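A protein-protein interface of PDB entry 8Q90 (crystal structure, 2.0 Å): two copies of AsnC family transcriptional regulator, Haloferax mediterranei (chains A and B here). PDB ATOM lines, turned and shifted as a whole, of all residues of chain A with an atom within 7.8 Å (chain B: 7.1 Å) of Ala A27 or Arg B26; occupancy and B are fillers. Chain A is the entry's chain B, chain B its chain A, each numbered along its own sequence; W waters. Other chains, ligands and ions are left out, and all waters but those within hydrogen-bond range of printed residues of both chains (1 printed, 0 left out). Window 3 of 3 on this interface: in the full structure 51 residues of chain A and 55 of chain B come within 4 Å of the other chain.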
ATOM      1  N   LEU A  17      -5.702   0.992   2.160  1.00  0.00           N
ATOM      2  CA  LEU A  17      -5.387   0.720   3.577  1.00  0.00           C
ATOM      3  C   LEU A  17      -5.644   1.990   4.399  1.00  0.00           C
ATOM      4  O   LEU A  17      -6.250   1.885   5.461  1.00  0.00           O
ATOM      5  CB  LEU A  17      -3.934   0.251   3.680  1.00  0.00           C
ATOM      6  CG  LEU A  17      -3.423   0.025   5.099  1.00  0.00           C
ATOM      7  CD1 LEU A  17      -4.309  -0.960   5.840  1.00  0.00           C
ATOM      8  CD2 LEU A  17      -1.983  -0.459   5.084  1.00  0.00           C
ATOM      9  N   ALA A  20      -9.246   2.539   4.727  1.00  0.00           N
ATOM     10  CA  ALA A  20      -9.860   1.573   5.666  1.00  0.00           C
ATOM     11  C   ALA A  20      -9.650   1.987   7.127  1.00  0.00           C
ATOM     12  O   ALA A  20     -10.539   1.762   7.935  1.00  0.00           O
ATOM     13  CB  ALA A  20      -9.293   0.210   5.397  1.00  0.00           C
ATOM     14  N   LEU A  21      -8.491   2.571   7.428  1.00  0.00           N
ATOM     15  CA  LEU A  21      -8.149   2.964   8.815  1.00  0.00           C
ATOM     16  C   LEU A  21      -8.894   4.248   9.196  1.00  0.00           C
ATOM     17  O   LEU A  21      -9.166   4.436  10.373  1.00  0.00           O
ATOM     18  CB  LEU A  21      -6.633   3.142   8.888  1.00  0.00           C
ATOM     19  CG  LEU A  21      -5.824   1.851   8.838  1.00  0.00           C
ATOM     20  CD1 LEU A  21      -4.394   2.132   8.417  1.00  0.00           C
ATOM     21  CD2 LEU A  21      -5.862   1.136  10.179  1.00  0.00           C
ATOM     22  N   GLY A  23     -11.470   6.577  10.352  1.00  0.00           N
ATOM     23  CA  GLY A  23     -12.657   6.257  11.167  1.00  0.00           C
ATOM     24  C   GLY A  23     -12.635   4.866  11.784  1.00  0.00           C
ATOM     25  O   GLY A  23     -13.550   4.585  12.548  1.00  0.00           O
ATOM     26  N   ASP A  24     -11.661   4.017  11.451  1.00  0.00           N
ATOM     27  CA  ASP A  24     -11.529   2.663  12.061  1.00  0.00           C
ATOM     28  C   ASP A  24     -10.053   2.379  12.335  1.00  0.00           C
ATOM     29  O   ASP A  24      -9.567   1.337  11.897  1.00  0.00           O
ATOM     30  CB  ASP A  24     -12.165   1.589  11.185  1.00  0.00           C
ATOM     31  CG  ASP A  24     -12.295   0.235  11.860  1.00  0.00           C
ATOM     32  OD1 ASP A  24     -12.220  -0.772  11.145  1.00  0.00           O
ATOM     33  OD2 ASP A  24     -12.467   0.198  13.087  1.00  0.00           O
ATOM     34  N   GLY A  25      -9.393   3.276  13.056  1.00  0.00           N
ATOM     35  CA  GLY A  25      -7.944   3.152  13.278  1.00  0.00           C
ATOM     36  C   GLY A  25      -7.527   2.087  14.271  1.00  0.00           C
ATOM     37  O   GLY A  25      -6.339   1.858  14.383  1.00  0.00           O
ATOM     38  N   ARG A  26      -8.468   1.456  14.956  1.00  0.00           N
ATOM     39  CA  ARG A  26      -8.063   0.357  15.864  1.00  0.00           C
ATOM     40  C   ARG A  26      -8.440  -0.994  15.242  1.00  0.00           C
ATOM     41  O   ARG A  26      -8.444  -1.993  15.959  1.00  0.00           O
ATOM     42  CB  ARG A  26      -8.644   0.611  17.255  1.00  0.00           C
ATOM     43  CG  ARG A  26      -7.804   1.528  18.129  1.00  0.00           C
ATOM     44  CD  ARG A  26      -8.312   1.567  19.556  1.00  0.00           C
ATOM     45  NE  ARG A  26      -8.031   0.345  20.296  1.00  0.00           N
ATOM     46  CZ  ARG A  26      -6.881   0.077  20.898  1.00  0.00           C
ATOM     47  NH1 ARG A  26      -5.889   0.947  20.851  1.00  0.00           N
ATOM     48  NH2 ARG A  26      -6.724  -1.062  21.545  1.00  0.00           N
ATOM     49  N   ALA A  27      -8.691  -1.009  13.938  1.00  0.00           N
ATOM     50  CA  ALA A  27      -8.992  -2.274  13.238  1.00  0.00           C
ATOM     51  C   ALA A  27      -7.841  -3.269  13.377  1.00  0.00           C
ATOM     52  O   ALA A  27      -6.689  -2.864  13.209  1.00  0.00           O
ATOM     53  CB  ALA A  27      -9.272  -2.010  11.795  1.00  0.00           C
ATOM     54  N   SER A  28      -8.176  -4.525  13.654  1.00  0.00           N
ATOM     55  CA  SER A  28      -7.162  -5.595  13.745  1.00  0.00           C
ATOM     56  C   SER A  28      -6.540  -5.862  12.380  1.00  0.00           C
ATOM     57  O   SER A  28      -7.204  -5.635  11.370  1.00  0.00           O
ATOM     58  CB  SER A  28      -7.791  -6.861  14.262  1.00  0.00           C
ATOM     59  OG  SER A  28      -8.603  -7.460  13.268  1.00  0.00           O
ATOM     60  N   LEU A  29      -5.312  -6.363  12.380  1.00  0.00           N
ATOM     61  CA  LEU A  29      -4.650  -6.753  11.117  1.00  0.00           C
ATOM     62  C   LEU A  29      -5.519  -7.781  10.384  1.00  0.00           C
ATOM     63  O   LEU A  29      -5.653  -7.658   9.179  1.00  0.00           O
ATOM     64  CB  LEU A  29      -3.276  -7.313  11.476  1.00  0.00           C
ATOM     65  CG  LEU A  29      -2.273  -6.285  11.993  1.00  0.00           C
ATOM     66  CD1 LEU A  29      -1.043  -6.968  12.559  1.00  0.00           C
ATOM     67  CD2 LEU A  29      -1.883  -5.312  10.894  1.00  0.00           C
ATOM     68  N   ARG A  30      -6.111  -8.724  11.114  1.00  0.00           N
ATOM     69  CA  ARG A  30      -6.965  -9.778  10.508  1.00  0.00           C
ATOM     70  C   ARG A  30      -8.148  -9.131   9.790  1.00  0.00           C
ATOM     71  O   ARG A  30      -8.429  -9.524   8.664  1.00  0.00           O
ATOM     72  CB  ARG A  30      -7.440 -10.740  11.600  1.00  0.00           C
ATOM     73  CG  ARG A  30      -8.249 -11.928  11.103  1.00  0.00           C
ATOM     74  CD  ARG A  30      -7.936 -13.139  11.958  1.00  0.00           C
ATOM     75  N   SER A  31      -8.790  -8.152  10.420  1.00  0.00           N
ATOM     76  CA  SER A  31      -9.938  -7.450   9.801  1.00  0.00           C
ATOM     77  C   SER A  31      -9.480  -6.661   8.566  1.00  0.00           C
ATOM     78  O   SER A  31     -10.119  -6.780   7.534  1.00  0.00           O
ATOM     79  CB  SER A  31     -10.651  -6.580  10.804  1.00  0.00           C
ATOM     80  OG  SER A  31     -11.069  -7.334  11.928  1.00  0.00           O
ATOM     81  N   LEU A  32      -8.402  -5.895   8.695  1.00  0.00           N
ATOM     82  CA  LEU A  32      -7.847  -5.111   7.563  1.00  0.00           C
ATOM     83  C   LEU A  32      -7.497  -6.055   6.411  1.00  0.00           C
ATOM     84  O   LEU A  32      -7.783  -5.724   5.264  1.00  0.00           O
ATOM     85  CB  LEU A  32      -6.614  -4.376   8.085  1.00  0.00           C
ATOM     86  CG  LEU A  32      -6.893  -3.238   9.065  1.00  0.00           C
ATOM     87  CD1 LEU A  32      -5.600  -2.698   9.652  1.00  0.00           C
ATOM     88  CD2 LEU A  32      -7.679  -2.124   8.393  1.00  0.00           C
ATOM     89  N   ALA A  33      -6.908  -7.195   6.741  1.00  0.00           N
ATOM     90  CA  ALA A  33      -6.519  -8.183   5.715  1.00  0.00           C
ATOM     91  C   ALA A  33      -7.776  -8.702   5.008  1.00  0.00           C
ATOM     92  O   ALA A  33      -7.792  -8.717   3.779  1.00  0.00           O
ATOM     93  CB  ALA A  33      -5.707  -9.273   6.362  1.00  0.00           C
ATOM     94  N   GLU A  35     -10.701  -7.212   4.859  1.00  0.00           N
ATOM     95  CA  GLU A  35     -11.284  -6.063   4.124  1.00  0.00           C
ATOM     96  C   GLU A  35     -10.567  -5.850   2.786  1.00  0.00           C
ATOM     97  O   GLU A  35     -11.255  -5.574   1.803  1.00  0.00           O
ATOM     98  CB  GLU A  35     -11.180  -4.805   4.977  1.00  0.00           C
ATOM     99  CG  GLU A  35     -12.368  -4.546   5.874  1.00  0.00           C
ATOM    100  CD  GLU A  35     -12.388  -3.122   6.397  1.00  0.00           C
ATOM    101  OE1 GLU A  35     -13.423  -2.451   6.246  1.00  0.00           O
ATOM    102  OE2 GLU A  35     -11.362  -2.684   6.941  1.00  0.00           O
ATOM    103  N   VAL A  43      -0.590  -6.580   5.098  1.00  0.00           N
ATOM    104  CA  VAL A  43      -1.058  -5.397   5.877  1.00  0.00           C
ATOM    105  C   VAL A  43       0.085  -4.890   6.768  1.00  0.00           C
ATOM    106  O   VAL A  43       0.454  -3.717   6.656  1.00  0.00           O
ATOM    107  CB  VAL A  43      -2.320  -5.720   6.699  1.00  0.00           C
ATOM    108  CG1 VAL A  43      -2.813  -4.516   7.479  1.00  0.00           C
ATOM    109  CG2 VAL A  43      -3.429  -6.278   5.826  1.00  0.00           C
ATOM    110  N   LEU A  47       1.690  -1.162   6.410  1.00  0.00           N
ATOM    111  CA  LEU A  47       1.486  -0.218   7.533  1.00  0.00           C
ATOM    112  C   LEU A  47       2.849   0.302   8.008  1.00  0.00           C
ATOM    113  O   LEU A  47       2.974   1.509   8.205  1.00  0.00           O
ATOM    114  CB  LEU A  47       0.731  -0.952   8.640  1.00  0.00           C
ATOM    115  CG  LEU A  47      -0.780  -0.738   8.666  1.00  0.00           C
ATOM    116  CD1 LEU A  47      -1.393  -1.383   9.896  1.00  0.00           C
ATOM    117  CD2 LEU A  47      -1.115   0.741   8.621  1.00  0.00           C
ATOM    118  N   GLU A  51       4.207   4.287   7.759  1.00  0.00           N
ATOM    119  CA  GLU A  51       4.618   4.988   9.001  1.00  0.00           C
ATOM    120  C   GLU A  51       6.090   5.389   8.870  1.00  0.00           C
ATOM    121  O   GLU A  51       6.412   6.522   9.191  1.00  0.00           O
ATOM    122  CB  GLU A  51       4.368   4.100  10.223  1.00  0.00           C
ATOM    123  CG  GLU A  51       2.913   3.749  10.471  1.00  0.00           C
ATOM    124  CD  GLU A  51       2.708   2.475  11.277  1.00  0.00           C
ATOM    125  OE1 GLU A  51       1.549   2.090  11.493  1.00  0.00           O
ATOM    126  OE2 GLU A  51       3.711   1.871  11.686  1.00  0.00           O
ATOM    127  N   ILE A  56       1.725   8.041   7.467  1.00  0.00           N
ATOM    128  CA  ILE A  56       0.957   7.866   8.691  1.00  0.00           C
ATOM    129  C   ILE A  56       1.851   8.331   9.826  1.00  0.00           C
ATOM    130  O   ILE A  56       2.910   7.745  10.073  1.00  0.00           O
ATOM    131  CB  ILE A  56       0.507   6.410   8.881  1.00  0.00           C
ATOM    132  CG1 ILE A  56      -0.415   5.982   7.732  1.00  0.00           C
ATOM    133  CG2 ILE A  56      -0.216   6.231  10.222  1.00  0.00           C
ATOM    134  CD1 ILE A  56      -0.694   4.487   7.697  1.00  0.00           C
ATOM    135  N   GLY A  58       0.878   8.571  13.037  1.00  0.00           N
ATOM    136  CA  GLY A  58       0.448   8.027  14.306  1.00  0.00           C
ATOM    137  C   GLY A  58      -1.049   7.858  14.302  1.00  0.00           C
ATOM    138  O   GLY A  58      -1.738   8.252  13.363  1.00  0.00           O
ATOM    139  N   TYR A  59      -1.511   7.226  15.367  1.00  0.00           N
ATOM    140  CA  TYR A  59      -2.946   6.931  15.495  1.00  0.00           C
ATOM    141  C   TYR A  59      -3.447   7.616  16.762  1.00  0.00           C
ATOM    142  O   TYR A  59      -2.688   7.768  17.717  1.00  0.00           O
ATOM    143  CB  TYR A  59      -3.140   5.418  15.498  1.00  0.00           C
ATOM    144  CG  TYR A  59      -2.550   4.708  14.308  1.00  0.00           C
ATOM    145  CD1 TYR A  59      -1.234   4.283  14.313  1.00  0.00           C
ATOM    146  CD2 TYR A  59      -3.305   4.470  13.173  1.00  0.00           C
ATOM    147  CE1 TYR A  59      -0.682   3.638  13.221  1.00  0.00           C
ATOM    148  CE2 TYR A  59      -2.768   3.826  12.072  1.00  0.00           C
ATOM    149  CZ  TYR A  59      -1.451   3.409  12.097  1.00  0.00           C
ATOM    150  OH  TYR A  59      -0.908   2.776  11.021  1.00  0.00           O
ATOM    151  N   THR A  60      -4.699   8.027  16.737  1.00  0.00           N
ATOM    152  CA  THR A  60      -5.229   8.764  17.896  1.00  0.00           C
ATOM    153  C   THR A  60      -6.737   8.609  18.010  1.00  0.00           C
ATOM    154  O   THR A  60      -7.406   8.385  17.003  1.00  0.00           O
ATOM    155  CB  THR A  60      -4.874  10.252  17.805  1.00  0.00           C
ATOM    156  OG1 THR A  60      -4.863  10.818  19.113  1.00  0.00           O
ATOM    157  CG2 THR A  60      -5.813  11.022  16.903  1.00  0.00           C
ATOM    158  N   PRO A  61      -7.283   8.716  19.230  1.00  0.00           N
ATOM    159  CA  PRO A  61      -8.718   8.716  19.382  1.00  0.00           C
ATOM    160  C   PRO A  61      -9.274  10.080  18.966  1.00  0.00           C
ATOM    161  O   PRO A  61      -8.550  11.026  19.053  1.00  0.00           O
ATOM    162  CB  PRO A  61      -8.876   8.550  20.894  1.00  0.00           C
ATOM    163  CG  PRO A  61      -7.625   9.142  21.480  1.00  0.00           C
ATOM    164  CD  PRO A  61      -6.548   8.771  20.490  1.00  0.00           C
ATOM    165  N   LEU B  21      -3.998   7.062  25.204  1.00  0.00           N
ATOM    166  CA  LEU B  21      -4.321   6.770  23.816  1.00  0.00           C
ATOM    167  C   LEU B  21      -3.857   7.877  22.881  1.00  0.00           C
ATOM    168  O   LEU B  21      -3.578   7.612  21.706  1.00  0.00           O
ATOM    169  CB  LEU B  21      -5.827   6.555  23.680  1.00  0.00           C
ATOM    170  CG  LEU B  21      -6.326   5.195  24.138  1.00  0.00           C
ATOM    171  CD1 LEU B  21      -7.794   5.246  24.376  1.00  0.00           C
ATOM    172  CD2 LEU B  21      -5.935   4.133  23.092  1.00  0.00           C
ATOM    173  N   GLY B  23      -1.798  10.161  20.704  1.00  0.00           N
ATOM    174  CA  GLY B  23      -0.545   9.814  20.061  1.00  0.00           C
ATOM    175  C   GLY B  23      -0.095   8.386  20.305  1.00  0.00           C
ATOM    176  O   GLY B  23       1.101   8.089  20.243  1.00  0.00           O
ATOM    177  N   ASP B  24      -1.035   7.494  20.625  1.00  0.00           N
ATOM    178  CA  ASP B  24      -0.721   6.072  20.713  1.00  0.00           C
ATOM    179  C   ASP B  24      -1.993   5.263  20.517  1.00  0.00           C
ATOM    180  O   ASP B  24      -2.236   4.278  21.223  1.00  0.00           O
ATOM    181  CB  ASP B  24      -0.050   5.731  22.047  1.00  0.00           C
ATOM    182  CG  ASP B  24       0.546   4.332  22.050  1.00  0.00           C
ATOM    183  OD1 ASP B  24       0.853   3.811  20.946  1.00  0.00           O
ATOM    184  OD2 ASP B  24       0.672   3.742  23.151  1.00  0.00           O
ATOM    185  N   GLY B  25      -2.781   5.669  19.518  1.00  0.00           N
ATOM    186  CA  GLY B  25      -4.146   5.203  19.353  1.00  0.00           C
ATOM    187  C   GLY B  25      -4.297   3.720  19.102  1.00  0.00           C
ATOM    188  O   GLY B  25      -5.397   3.181  19.294  1.00  0.00           O
ATOM    189  N   ARG B  26      -3.236   3.042  18.668  1.00  0.00           N
ATOM    190  CA  ARG B  26      -3.322   1.616  18.371  1.00  0.00           C
ATOM    191  C   ARG B  26      -2.651   0.736  19.423  1.00  0.00           C
ATOM    192  O   ARG B  26      -2.463  -0.464  19.189  1.00  0.00           O
ATOM    193  CB  ARG B  26      -2.743   1.340  16.981  1.00  0.00           C
ATOM    194  CG  ARG B  26      -3.820   1.357  15.902  1.00  0.00           C
ATOM    195  CD  ARG B  26      -3.252   1.137  14.497  1.00  0.00           C
ATOM    196  NE  ARG B  26      -3.063  -0.270  14.160  1.00  0.00           N
ATOM    197  CZ  ARG B  26      -4.012  -1.067  13.693  1.00  0.00           C
ATOM    198  NH1 ARG B  26      -5.237  -0.609  13.494  1.00  0.00           N
ATOM    199  NH2 ARG B  26      -3.730  -2.330  13.430  1.00  0.00           N
ATOM    200  N   ALA B  27      -2.314   1.288  20.581  1.00  0.00           N
ATOM    201  CA  ALA B  27      -1.744   0.490  21.653  1.00  0.00           C
ATOM    202  C   ALA B  27      -2.644  -0.687  21.988  1.00  0.00           C
ATOM    203  O   ALA B  27      -3.856  -0.537  22.125  1.00  0.00           O
ATOM    204  CB  ALA B  27      -1.536   1.357  22.897  1.00  0.00           C
ATOM    205  N   SER B  28      -2.005  -1.832  22.202  1.00  0.00           N
ATOM    206  CA  SER B  28      -2.731  -3.048  22.611  1.00  0.00           C
ATOM    207  C   SER B  28      -3.391  -2.820  23.974  1.00  0.00           C
ATOM    208  O   SER B  28      -2.901  -1.981  24.725  1.00  0.00           O
ATOM    209  CB  SER B  28      -1.774  -4.199  22.664  1.00  0.00           C
ATOM    210  OG  SER B  28      -0.789  -4.002  23.656  1.00  0.00           O
ATOM    211  N   LEU B  29      -4.468  -3.548  24.250  1.00  0.00           N
ATOM    212  CA  LEU B  29      -5.148  -3.476  25.567  1.00  0.00           C
ATOM    213  C   LEU B  29      -4.148  -3.878  26.654  1.00  0.00           C
ATOM    214  O   LEU B  29      -4.164  -3.264  27.701  1.00  0.00           O
ATOM    215  CB  LEU B  29      -6.356  -4.409  25.521  1.00  0.00           C
ATOM    216  CG  LEU B  29      -7.515  -4.005  24.616  1.00  0.00           C
ATOM    217  CD1 LEU B  29      -8.529  -5.132  24.532  1.00  0.00           C
ATOM    218  CD2 LEU B  29      -8.179  -2.733  25.117  1.00  0.00           C
ATOM    219  N   SER B  31      -0.778  -3.455  26.541  1.00  0.00           N
ATOM    220  CA  SER B  31       0.126  -2.287  26.711  1.00  0.00           C
ATOM    221  C   SER B  31      -0.561  -1.200  27.545  1.00  0.00           C
ATOM    222  O   SER B  31       0.005  -0.814  28.571  1.00  0.00           O
ATOM    223  CB  SER B  31       0.590  -1.757  25.382  1.00  0.00           C
ATOM    224  OG  SER B  31       1.107  -0.446  25.516  1.00  0.00           O
ATOM    225  N   LEU B  32      -1.825  -0.904  27.232  1.00  0.00           N
ATOM    226  CA  LEU B  32      -2.583   0.127  27.989  1.00  0.00           C
ATOM    227  C   LEU B  32      -2.749  -0.332  29.442  1.00  0.00           C
ATOM    228  O   LEU B  32      -2.500   0.466  30.340  1.00  0.00           O
ATOM    229  CB  LEU B  32      -3.928   0.337  27.295  1.00  0.00           C
ATOM    230  CG  LEU B  32      -3.851   0.987  25.916  1.00  0.00           C
ATOM    231  CD1 LEU B  32      -5.105   0.693  25.113  1.00  0.00           C
ATOM    232  CD2 LEU B  32      -3.625   2.483  26.042  1.00  0.00           C
ATOM    233  N   TYR B  59     -11.521   6.136  16.329  1.00  0.00           N
ATOM    234  CA  TYR B  59     -10.047   6.172  16.247  1.00  0.00           C
ATOM    235  C   TYR B  59      -9.645   6.397  14.791  1.00  0.00           C
ATOM    236  O   TYR B  59     -10.330   5.912  13.889  1.00  0.00           O
ATOM    237  CB  TYR B  59      -9.469   4.899  16.864  1.00  0.00           C
ATOM    238  CG  TYR B  59      -9.912   4.619  18.274  1.00  0.00           C
ATOM    239  CD1 TYR B  59     -11.047   3.869  18.524  1.00  0.00           C
ATOM    240  CD2 TYR B  59      -9.196   5.096  19.356  1.00  0.00           C
ATOM    241  CE1 TYR B  59     -11.462   3.602  19.815  1.00  0.00           C
ATOM    242  CE2 TYR B  59      -9.598   4.841  20.655  1.00  0.00           C
ATOM    243  CZ  TYR B  59     -10.735   4.090  20.884  1.00  0.00           C
ATOM    244  OH  TYR B  59     -11.143   3.829  22.154  1.00  0.00           O
ATOM    245  N   PRO B  61      -5.994   7.352  11.953  1.00  0.00           N
ATOM    246  CA  PRO B  61      -4.586   7.645  11.775  1.00  0.00           C
ATOM    247  C   PRO B  61      -4.383   9.140  11.517  1.00  0.00           C
ATOM    248  O   PRO B  61      -5.275   9.759  11.013  1.00  0.00           O
ATOM    249  CB  PRO B  61      -4.242   6.835  10.531  1.00  0.00           C
ATOM    250  CG  PRO B  61      -5.523   6.806   9.738  1.00  0.00           C
ATOM    251  CD  PRO B  61      -6.607   6.717  10.788  1.00  0.00           C
HETATM  252  O   HOH W   1     -13.010   3.943  14.956  1.00  0.00           O
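Among the printed residues, merely in contact across the chains: Gly A23 with Tyr B59, Gly A58 with Pro B61, Pro A61 with Leu B21, Leu A21 with Pro B61, Thr A60 with Gly B23, Thr A60 with Tyr B59, Arg A26 with Arg B26, Tyr A59 with Arg B26, Arg A26 with Tyr B59, Pro A61 with Tyr B59, Tyr A59 with Pro B61, Tyr A59 with Gly B23, Leu A21 with Arg B26, Thr A60 with Gly B25, Arg A26 with Leu B21 and Leu A21 with Tyr B59.
The backbone carbonyl oxygen of Tyr A59 is in hydrogen-bond range of the backbone NH of Asp B24. The backbone carbonyl oxygen (O) of Gly B25 lies within hydrogen-bond range of the guanidinium group (NH1) of Arg A26 (2.8 Å). The backbone NH (N) of Gly B25 sits at hydrogen-bond distance from the backbone carbonyl oxygen (O) of Tyr A59, at 2.8 Å. NH1 of Arg B26 is in hydrogen-bond range of O of Gly A25 (2.8 Å). The guanidinium group (NH1) of Arg B26 is in hydrogen-bond range of the backbone carbonyl oxygen (O) of Ala A27. O of Ala B27 sits at hydrogen-bond distance from NH1 of Arg A26, at 2.8 Å. O of Tyr B59 sits at hydrogen-bond distance from N of Asp A24, 3.4 Å away. O of Tyr B59 lies within hydrogen-bond range of N of Gly A25 (2.9 Å).
The side-chain carboxylate (OE1) of Glu A51 sits at hydrogen-bond distance from the side-chain hydroxyl (OH) of Tyr A59 (2.6 Å).
Leu A21 touches Tyr B59, but with the chains exchanged Tyr A59 does not touch Leu B21 (4.1 Å). Gly A23 touches Tyr B59, and with the chains exchanged Tyr A59 touches Gly B23. Arg A26 touches Tyr B59, and with the chains exchanged Tyr A59 touches Arg B26. Tyr A59 touches Pro B61, and with the chains exchanged Pro A61 touches Tyr B59. Of the 24 pairs that touch across the chains among the printed residues, 19 have their exchanged pair printed and touching as well.
Of chain B, only Arg B26 (2.7 Å) comes within 4 Å of Ala A27. Of chain A, only Leu A21 (3.8 Å), Gly A25 (2.8 Å), Arg A26 (3.5 Å), Ala A27 (2.7 Å) and Tyr A59 (3.6 Å) come within 4 Å of Arg B26. Gly B25 touches just these residues of chain A: Arg A26 (2.8 Å), Tyr A59 (2.8 Å) and Thr A60 (3.9 Å). Of the printed residues of chain B, Thr A60 touches Gly B23 (3.5 Å), Gly B25 (3.9 Å) and Tyr B59 (3.5 Å). Of the printed residues of chain B, Tyr A59 touches Gly B23, Asp B24, Gly B25, Arg B26 and Pro B61. Leu A32 touches none of the printed residues of chain B.
Water W1 lies within hydrogen-bond range of O of Gly A23 (2.5 Å) and N of Tyr B59 (3.0 Å).
Of the 12 printed residues of chain B, 8 touch a printed residue of chain A. Printed residues of chain B that touch a printed residue of chain A: Leu B21, Gly B23, Asp B24, Gly B25, Arg B26, Ala B27, Tyr B59 and Pro B61. Among the printed residues, no Asp or Glu carboxylate lies within 4 Å of a Lys or Arg side-chain nitrogen of the other chain.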
